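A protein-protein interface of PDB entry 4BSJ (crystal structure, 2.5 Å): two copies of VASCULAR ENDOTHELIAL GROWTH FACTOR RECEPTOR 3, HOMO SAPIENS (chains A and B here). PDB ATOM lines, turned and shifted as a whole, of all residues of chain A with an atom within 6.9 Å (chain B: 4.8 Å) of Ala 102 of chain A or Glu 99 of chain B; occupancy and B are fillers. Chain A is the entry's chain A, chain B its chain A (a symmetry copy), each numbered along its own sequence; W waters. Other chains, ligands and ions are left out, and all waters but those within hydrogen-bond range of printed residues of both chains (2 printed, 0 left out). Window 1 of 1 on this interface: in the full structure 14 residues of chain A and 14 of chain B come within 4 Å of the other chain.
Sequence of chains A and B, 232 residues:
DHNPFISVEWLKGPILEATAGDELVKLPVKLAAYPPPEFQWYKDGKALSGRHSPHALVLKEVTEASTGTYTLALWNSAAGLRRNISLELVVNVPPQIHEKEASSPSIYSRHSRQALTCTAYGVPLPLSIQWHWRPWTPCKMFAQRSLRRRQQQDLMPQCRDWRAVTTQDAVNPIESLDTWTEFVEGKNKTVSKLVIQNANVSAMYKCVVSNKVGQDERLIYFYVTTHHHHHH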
ATOM      1  N   ILE A  97     -12.915  -7.441  25.193  1.00  0.00           N
ATOM      2  CA  ILE A  97     -13.814  -8.538  25.505  1.00  0.00           C
ATOM      3  C   ILE A  97     -14.794  -8.699  24.359  1.00  0.00           C
ATOM      4  O   ILE A  97     -15.616  -7.822  24.108  1.00  0.00           O
ATOM      5  CB  ILE A  97     -14.573  -8.283  26.792  1.00  0.00           C
ATOM      6  CG1 ILE A  97     -13.590  -8.178  27.959  1.00  0.00           C
ATOM      7  CG2 ILE A  97     -15.581  -9.386  27.033  1.00  0.00           C
ATOM      8  CD1 ILE A  97     -14.195  -7.612  29.220  1.00  0.00           C
ATOM      9  N   HIS A  98     -14.705  -9.828  23.664  1.00  0.00           N
ATOM     10  CA  HIS A  98     -15.412  -9.988  22.397  1.00  0.00           C
ATOM     11  C   HIS A  98     -16.922 -10.130  22.489  1.00  0.00           C
ATOM     12  O   HIS A  98     -17.630  -9.727  21.568  1.00  0.00           O
ATOM     13  CB  HIS A  98     -14.796 -11.128  21.585  1.00  0.00           C
ATOM     14  CG  HIS A  98     -13.358 -10.895  21.264  1.00  0.00           C
ATOM     15  ND1 HIS A  98     -12.351 -11.730  21.694  1.00  0.00           N
ATOM     16  CD2 HIS A  98     -12.752  -9.878  20.607  1.00  0.00           C
ATOM     17  CE1 HIS A  98     -11.188 -11.253  21.288  1.00  0.00           C
ATOM     18  NE2 HIS A  98     -11.403 -10.132  20.625  1.00  0.00           N
ATOM     19  N   GLU A  99     -17.417 -10.684  23.594  1.00  0.00           N
ATOM     20  CA  GLU A  99     -18.857 -10.884  23.756  1.00  0.00           C
ATOM     21  C   GLU A  99     -19.621  -9.569  23.709  1.00  0.00           C
ATOM     22  O   GLU A  99     -20.814  -9.556  23.415  1.00  0.00           O
ATOM     23  CB  GLU A  99     -19.180 -11.634  25.050  1.00  0.00           C
ATOM     24  CG  GLU A  99     -18.947 -13.141  24.978  1.00  0.00           C
ATOM     25  CD  GLU A  99     -17.504 -13.529  25.249  1.00  0.00           C
ATOM     26  OE1 GLU A  99     -16.640 -12.632  25.329  1.00  0.00           O
ATOM     27  OE2 GLU A  99     -17.238 -14.739  25.391  1.00  0.00           O
ATOM     28  N   LYS A 100     -18.918  -8.474  23.986  1.00  0.00           N
ATOM     29  CA  LYS A 100     -19.486  -7.132  23.922  1.00  0.00           C
ATOM     30  C   LYS A 100     -19.996  -6.797  22.538  1.00  0.00           C
ATOM     31  O   LYS A 100     -20.973  -6.070  22.397  1.00  0.00           O
ATOM     32  CB  LYS A 100     -18.447  -6.085  24.318  1.00  0.00           C
ATOM     33  CG  LYS A 100     -18.056  -6.117  25.773  1.00  0.00           C
ATOM     34  CD  LYS A 100     -17.015  -5.064  26.065  1.00  0.00           C
ATOM     35  CE  LYS A 100     -17.578  -3.673  25.856  1.00  0.00           C
ATOM     36  NZ  LYS A 100     -16.685  -2.640  26.436  1.00  0.00           N
ATOM     37  N   GLU A 101     -19.328  -7.323  21.519  1.00  0.00           N
ATOM     38  CA  GLU A 101     -19.670  -7.008  20.135  1.00  0.00           C
ATOM     39  C   GLU A 101     -20.882  -7.793  19.642  1.00  0.00           C
ATOM     40  O   GLU A 101     -21.413  -7.532  18.566  1.00  0.00           O
ATOM     41  CB  GLU A 101     -18.477  -7.300  19.233  1.00  0.00           C
ATOM     42  CG  GLU A 101     -17.330  -6.327  19.384  1.00  0.00           C
ATOM     43  CD  GLU A 101     -17.458  -5.149  18.437  1.00  0.00           C
ATOM     44  OE1 GLU A 101     -18.314  -4.264  18.681  1.00  0.00           O
ATOM     45  OE2 GLU A 101     -16.705  -5.116  17.438  1.00  0.00           O
ATOM     46  N   ALA A 102     -21.314  -8.765  20.430  1.00  0.00           N
ATOM     47  CA  ALA A 102     -22.367  -9.660  19.995  1.00  0.00           C
ATOM     48  C   ALA A 102     -23.643  -9.414  20.784  1.00  0.00           C
ATOM     49  O   ALA A 102     -23.609  -8.881  21.892  1.00  0.00           O
ATOM     50  CB  ALA A 102     -21.919 -11.102  20.146  1.00  0.00           C
ATOM     51  N   SER A 103     -24.769  -9.805  20.207  1.00  0.00           N
ATOM     52  CA  SER A 103     -26.037  -9.705  20.907  1.00  0.00           C
ATOM     53  C   SER A 103     -25.989 -10.446  22.242  1.00  0.00           C
ATOM     54  O   SER A 103     -25.199 -11.372  22.435  1.00  0.00           O
ATOM     55  CB  SER A 103     -27.165 -10.252  20.041  1.00  0.00           C
ATOM     56  OG  SER A 103     -28.332 -10.436  20.810  1.00  0.00           O
ATOM     57  N   SER A 104     -26.837 -10.026  23.167  1.00  0.00           N
ATOM     58  CA  SER A 104     -26.849 -10.597  24.496  1.00  0.00           C
ATOM     59  C   SER A 104     -28.292 -10.629  24.968  1.00  0.00           C
ATOM     60  O   SER A 104     -29.061  -9.715  24.673  1.00  0.00           O
ATOM     61  CB  SER A 104     -25.983  -9.748  25.427  1.00  0.00           C
ATOM     62  OG  SER A 104     -25.887 -10.319  26.718  1.00  0.00           O
ATOM     63  N   VAL A 184      -8.714 -19.438  19.604  1.00  0.00           N
ATOM     64  CA  VAL A 184      -9.887 -18.923  18.912  1.00  0.00           C
ATOM     65  C   VAL A 184      -9.435 -18.008  17.785  1.00  0.00           C
ATOM     66  O   VAL A 184      -8.671 -17.068  18.015  1.00  0.00           O
ATOM     67  CB  VAL A 184     -10.801 -18.098  19.856  1.00  0.00           C
ATOM     68  CG1 VAL A 184     -12.046 -17.648  19.118  1.00  0.00           C
ATOM     69  CG2 VAL A 184     -11.171 -18.889  21.116  1.00  0.00           C
ATOM     70  N   GLU A 185      -9.908 -18.291  16.574  1.00  0.00           N
ATOM     71  CA  GLU A 185      -9.587 -17.497  15.388  1.00  0.00           C
ATOM     72  C   GLU A 185      -8.100 -17.178  15.248  1.00  0.00           C
ATOM     73  O   GLU A 185      -7.721 -16.028  15.029  1.00  0.00           O
ATOM     74  CB  GLU A 185     -10.408 -16.206  15.354  1.00  0.00           C
ATOM     75  CG  GLU A 185     -11.885 -16.421  15.080  1.00  0.00           C
ATOM     76  CD  GLU A 185     -12.164 -16.867  13.657  1.00  0.00           C
ATOM     77  OE1 GLU A 185     -11.803 -16.123  12.718  1.00  0.00           O
ATOM     78  OE2 GLU A 185     -12.751 -17.958  13.480  1.00  0.00           O
ATOM     79  N   ARG A 218     -17.188  -5.661  30.431  1.00  0.00           N
ATOM     80  CA  ARG A 218     -18.463  -6.005  29.827  1.00  0.00           C
ATOM     81  C   ARG A 218     -19.515  -6.045  30.919  1.00  0.00           C
ATOM     82  O   ARG A 218     -19.353  -6.753  31.926  1.00  0.00           O
ATOM     83  CB  ARG A 218     -18.395  -7.347  29.099  1.00  0.00           C
ATOM     84  CG  ARG A 218     -19.722  -7.783  28.490  1.00  0.00           C
ATOM     85  CD  ARG A 218     -19.754  -9.291  28.239  1.00  0.00           C
ATOM     86  NE  ARG A 218     -21.008  -9.722  27.629  1.00  0.00           N
ATOM     87  CZ  ARG A 218     -21.506 -10.952  27.722  1.00  0.00           C
ATOM     88  NH1 ARG A 218     -20.863 -11.885  28.408  1.00  0.00           N
ATOM     89  NH2 ARG A 218     -22.655 -11.251  27.132  1.00  0.00           N
ATOM     90  N   ILE B  97     -19.174 -12.007  11.511  1.00  0.00           N
ATOM     91  CA  ILE B  97     -19.983 -12.620  12.552  1.00  0.00           C
ATOM     92  C   ILE B  97     -19.181 -12.637  13.839  1.00  0.00           C
ATOM     93  O   ILE B  97     -18.164 -13.320  13.936  1.00  0.00           O
ATOM     94  CB  ILE B  97     -20.381 -14.034  12.181  1.00  0.00           C
ATOM     95  CG1 ILE B  97     -21.239 -14.013  10.915  1.00  0.00           C
ATOM     96  CG2 ILE B  97     -21.126 -14.685  13.328  1.00  0.00           C
ATOM     97  CD1 ILE B  97     -21.424 -15.369  10.279  1.00  0.00           C
ATOM     98  N   HIS B  98     -19.642 -11.882  14.830  1.00  0.00           N
ATOM     99  CA  HIS B  98     -18.833 -11.619  16.015  1.00  0.00           C
ATOM    100  C   HIS B  98     -18.635 -12.790  16.961  1.00  0.00           C
ATOM    101  O   HIS B  98     -17.603 -12.869  17.626  1.00  0.00           O
ATOM    102  CB  HIS B  98     -19.359 -10.389  16.756  1.00  0.00           C
ATOM    103  CG  HIS B  98     -19.332  -9.155  15.917  1.00  0.00           C
ATOM    104  ND1 HIS B  98     -20.468  -8.448  15.589  1.00  0.00           N
ATOM    105  CD2 HIS B  98     -18.308  -8.539  15.284  1.00  0.00           C
ATOM    106  CE1 HIS B  98     -20.140  -7.432  14.813  1.00  0.00           C
ATOM    107  NE2 HIS B  98     -18.834  -7.463  14.614  1.00  0.00           N
ATOM    108  N   GLU B  99     -19.605 -13.701  17.015  1.00  0.00           N
ATOM    109  CA  GLU B  99     -19.509 -14.849  17.918  1.00  0.00           C
ATOM    110  C   GLU B  99     -18.297 -15.714  17.611  1.00  0.00           C
ATOM    111  O   GLU B  99     -17.825 -16.449  18.475  1.00  0.00           O
ATOM    112  CB  GLU B  99     -20.783 -15.697  17.888  1.00  0.00           C
ATOM    113  CG  GLU B  99     -21.943 -15.118  18.693  1.00  0.00           C
ATOM    114  CD  GLU B  99     -22.747 -14.090  17.917  1.00  0.00           C
ATOM    115  OE1 GLU B  99     -22.318 -13.694  16.814  1.00  0.00           O
ATOM    116  OE2 GLU B  99     -23.817 -13.685  18.412  1.00  0.00           O
ATOM    117  N   LYS B 100     -17.798 -15.607  16.382  1.00  0.00           N
ATOM    118  CA  LYS B 100     -16.600 -16.319  15.949  1.00  0.00           C
ATOM    119  C   LYS B 100     -15.391 -15.953  16.778  1.00  0.00           C
ATOM    120  O   LYS B 100     -14.518 -16.784  17.001  1.00  0.00           O
ATOM    121  CB  LYS B 100     -16.291 -16.015  14.484  1.00  0.00           C
ATOM    122  CG  LYS B 100     -17.285 -16.587  13.506  1.00  0.00           C
ATOM    123  CD  LYS B 100     -16.908 -16.220  12.092  1.00  0.00           C
ATOM    124  CE  LYS B 100     -15.589 -16.854  11.702  1.00  0.00           C
ATOM    125  NZ  LYS B 100     -15.364 -16.768  10.237  1.00  0.00           N
ATOM    126  N   GLU B 101     -15.337 -14.704  17.225  1.00  0.00           N
ATOM    127  CA  GLU B 101     -14.182 -14.205  17.965  1.00  0.00           C
ATOM    128  C   GLU B 101     -14.193 -14.644  19.426  1.00  0.00           C
ATOM    129  O   GLU B 101     -13.219 -14.462  20.152  1.00  0.00           O
ATOM    130  CB  GLU B 101     -14.147 -12.684  17.895  1.00  0.00           C
ATOM    131  CG  GLU B 101     -13.772 -12.132  16.539  1.00  0.00           C
ATOM    132  CD  GLU B 101     -12.272 -11.938  16.401  1.00  0.00           C
ATOM    133  OE1 GLU B 101     -11.541 -12.948  16.255  1.00  0.00           O
ATOM    134  OE2 GLU B 101     -11.826 -10.771  16.451  1.00  0.00           O
ATOM    135  N   ALA B 102     -15.305 -15.217  19.860  1.00  0.00           N
ATOM    136  CA  ALA B 102     -15.472 -15.545  21.262  1.00  0.00           C
ATOM    137  C   ALA B 102     -15.455 -17.050  21.469  1.00  0.00           C
ATOM    138  O   ALA B 102     -15.724 -17.820  20.549  1.00  0.00           O
ATOM    139  CB  ALA B 102     -16.769 -14.953  21.784  1.00  0.00           C
ATOM    140  N   THR B 117     -26.666 -18.377  18.339  1.00  0.00           N
ATOM    141  CA  THR B 117     -26.840 -16.975  18.004  1.00  0.00           C
ATOM    142  C   THR B 117     -25.730 -16.454  17.113  1.00  0.00           C
ATOM    143  O   THR B 117     -24.552 -16.672  17.377  1.00  0.00           O
ATOM    144  CB  THR B 117     -26.903 -16.110  19.282  1.00  0.00           C
ATOM    145  OG1 THR B 117     -27.991 -16.555  20.102  1.00  0.00           O
ATOM    146  CG2 THR B 117     -27.109 -14.650  18.934  1.00  0.00           C
ATOM    147  N   CYS B 118     -26.114 -15.761  16.050  1.00  0.00           N
ATOM    148  CA  CYS B 118     -25.137 -15.112  15.195  1.00  0.00           C
ATOM    149  C   CYS B 118     -25.432 -13.628  15.063  1.00  0.00           C
ATOM    150  O   CYS B 118     -26.554 -13.227  14.732  1.00  0.00           O
ATOM    151  CB  CYS B 118     -25.078 -15.789  13.827  1.00  0.00           C
ATOM    152  SG  CYS B 118     -24.284 -17.432  13.882  1.00  0.00           S
ATOM    153  N   THR B 119     -24.414 -12.822  15.345  1.00  0.00           N
ATOM    154  CA  THR B 119     -24.523 -11.376  15.256  1.00  0.00           C
ATOM    155  C   THR B 119     -23.588 -10.880  14.169  1.00  0.00           C
ATOM    156  O   THR B 119     -22.386 -11.159  14.194  1.00  0.00           O
ATOM    157  CB  THR B 119     -24.172 -10.695  16.590  1.00  0.00           C
ATOM    158  OG1 THR B 119     -24.998 -11.229  17.632  1.00  0.00           O
ATOM    159  CG2 THR B 119     -24.396  -9.191  16.497  1.00  0.00           C
ATOM    160  N   VAL B 184     -25.951  -2.588  19.139  1.00  0.00           N
ATOM    161  CA  VAL B 184     -24.861  -3.187  19.898  1.00  0.00           C
ATOM    162  C   VAL B 184     -23.593  -2.381  19.663  1.00  0.00           C
ATOM    163  O   VAL B 184     -23.199  -2.160  18.516  1.00  0.00           O
ATOM    164  CB  VAL B 184     -24.583  -4.648  19.456  1.00  0.00           C
ATOM    165  CG1 VAL B 184     -23.497  -5.258  20.322  1.00  0.00           C
ATOM    166  CG2 VAL B 184     -25.855  -5.502  19.497  1.00  0.00           C
ATOM    167  N   ARG B 218     -19.951 -18.843  10.272  1.00  0.00           N
ATOM    168  CA  ARG B 218     -19.543 -19.367  11.563  1.00  0.00           C
ATOM    169  C   ARG B 218     -19.981 -20.818  11.650  1.00  0.00           C
ATOM    170  O   ARG B 218     -21.165 -21.134  11.452  1.00  0.00           O
ATOM    171  CB  ARG B 218     -20.144 -18.558  12.712  1.00  0.00           C
ATOM    172  CG  ARG B 218     -19.791 -19.098  14.093  1.00  0.00           C
ATOM    173  CD  ARG B 218     -20.782 -18.613  15.153  1.00  0.00           C
ATOM    174  NE  ARG B 218     -20.442 -19.097  16.487  1.00  0.00           N
ATOM    175  CZ  ARG B 218     -21.316 -19.241  17.480  1.00  0.00           C
ATOM    176  NH1 ARG B 218     -22.594 -18.943  17.295  1.00  0.00           N
ATOM    177  NH2 ARG B 218     -20.913 -19.689  18.660  1.00  0.00           N
HETATM  178  O   HOH W   1     -18.310 -11.992  20.146  1.00  0.00           O
HETATM  179  O   HOH W   2     -24.172 -14.192  20.976  1.00  0.00           O
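ND1 of His 98 of chain A is in hydrogen-bond range of O of Glu 101 of chain B (3.3 Å). O of Glu 101 of chain A lies within hydrogen-bond range of ND1 of His 98 of chain B. N of Ser 103 of chain A sits at hydrogen-bond distance from OG1 of Thr 119 of chain B (3.0 Å).
O of Thr 119 of chain B lies within hydrogen-bond range of N of His 98 of chain B. OE1 of Glu 99 of chain B sits at hydrogen-bond distance from N of Thr 119 of chain B (2.7 Å).
Glu 99 of chain A touches Ala 102 of chain B. Lys 100 of chain A touches Val 184 of chain B (O to CG1, 3.4 Å). Thr 119 of chain B touches Glu 101 of chain A (CG2 to O, 3.99 Å). Val 184 of chain B touches Glu 101 of chain A (CG1 to O, 3.5 Å). OE2 of Glu 99 of chain B touches CB of Ala 102 of chain A, 3.6 Å away. Lys 100 of chain B touches Val 184 of chain A. Val 184 of chain A touches Glu 101 of chain B (CG1 to O, 3.5 Å). Val 184 of chain A touches Ala 102 of chain B. O of Lys 100 of chain B touches CG of Glu 185 of chain A, 3.3 Å away. Glu 185 of chain A touches Glu 101 of chain B.
Ala 102 of chain A touches just these residues of chain B: Glu 99, Thr 119 and Val 184. Of chain A, only Ala 102 (3.6 Å) comes within 4 Å of Glu 99 of chain B. Printed residues of chain A within 4 Å of Lys 100 of chain B: Val 184 (3.4 Å) and Glu 185 (3.3 Å). Of the printed residues of chain A, Ala 102 of chain B touches Glu 99 and Val 184. Printed residues of chain B within 4 Å of Lys 100 of chain A: Val 184. Arg 218 of chain A touches none of the printed residues of chain B.
Of the 11 printed residues of chain A, 8 touch a printed residue of chain B. Printed residues of chain A that touch a printed residue of chain B: His 98, Glu 99, Lys 100, Glu 101, Ala 102, Ser 103, Val 184 and Glu 185. Along chain A the printed residues that touch a printed residue of chain B span positions 98 to 185. Hydrophobic or aromatic side chains of chain B that line the printed part of chain A: His 98, Ala 102 and Val 184. Among the printed residues, 15 pairs touch across the chains. Among the printed residues, no Asp or Glu carboxylate lies within 4 Å of a Lys or Arg side-chain nitrogen of the other chain.
His 98 of chain A touches Glu 101 of chain B, and with the chains exchanged Glu 101 of chain A touches His 98 of chain B. Glu 99 of chain A touches Ala 102 of chain B, and with the chains exchanged Ala 102 of chain A touches Glu 99 of chain B. Glu 101 of chain A touches Val 184 of chain B, and with the chains exchanged Val 184 of chain A touches Glu 101 of chain B. Ala 102 of chain A touches Val 184 of chain B, and with the chains exchanged Val 184 of chain A touches Ala 102 of chain B. 8 positions are printed for both chains.
Water W2 lies within hydrogen-bond range of OE2 of Glu 99 of chain B (2.6 Å) and O of Ser 103 of chain A (3.3 Å). Water W1 lies within hydrogen-bond range of the backbone carbonyl oxygen of His 98 of chain A and the backbone carbonyl oxygen of His 98 of chain B.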
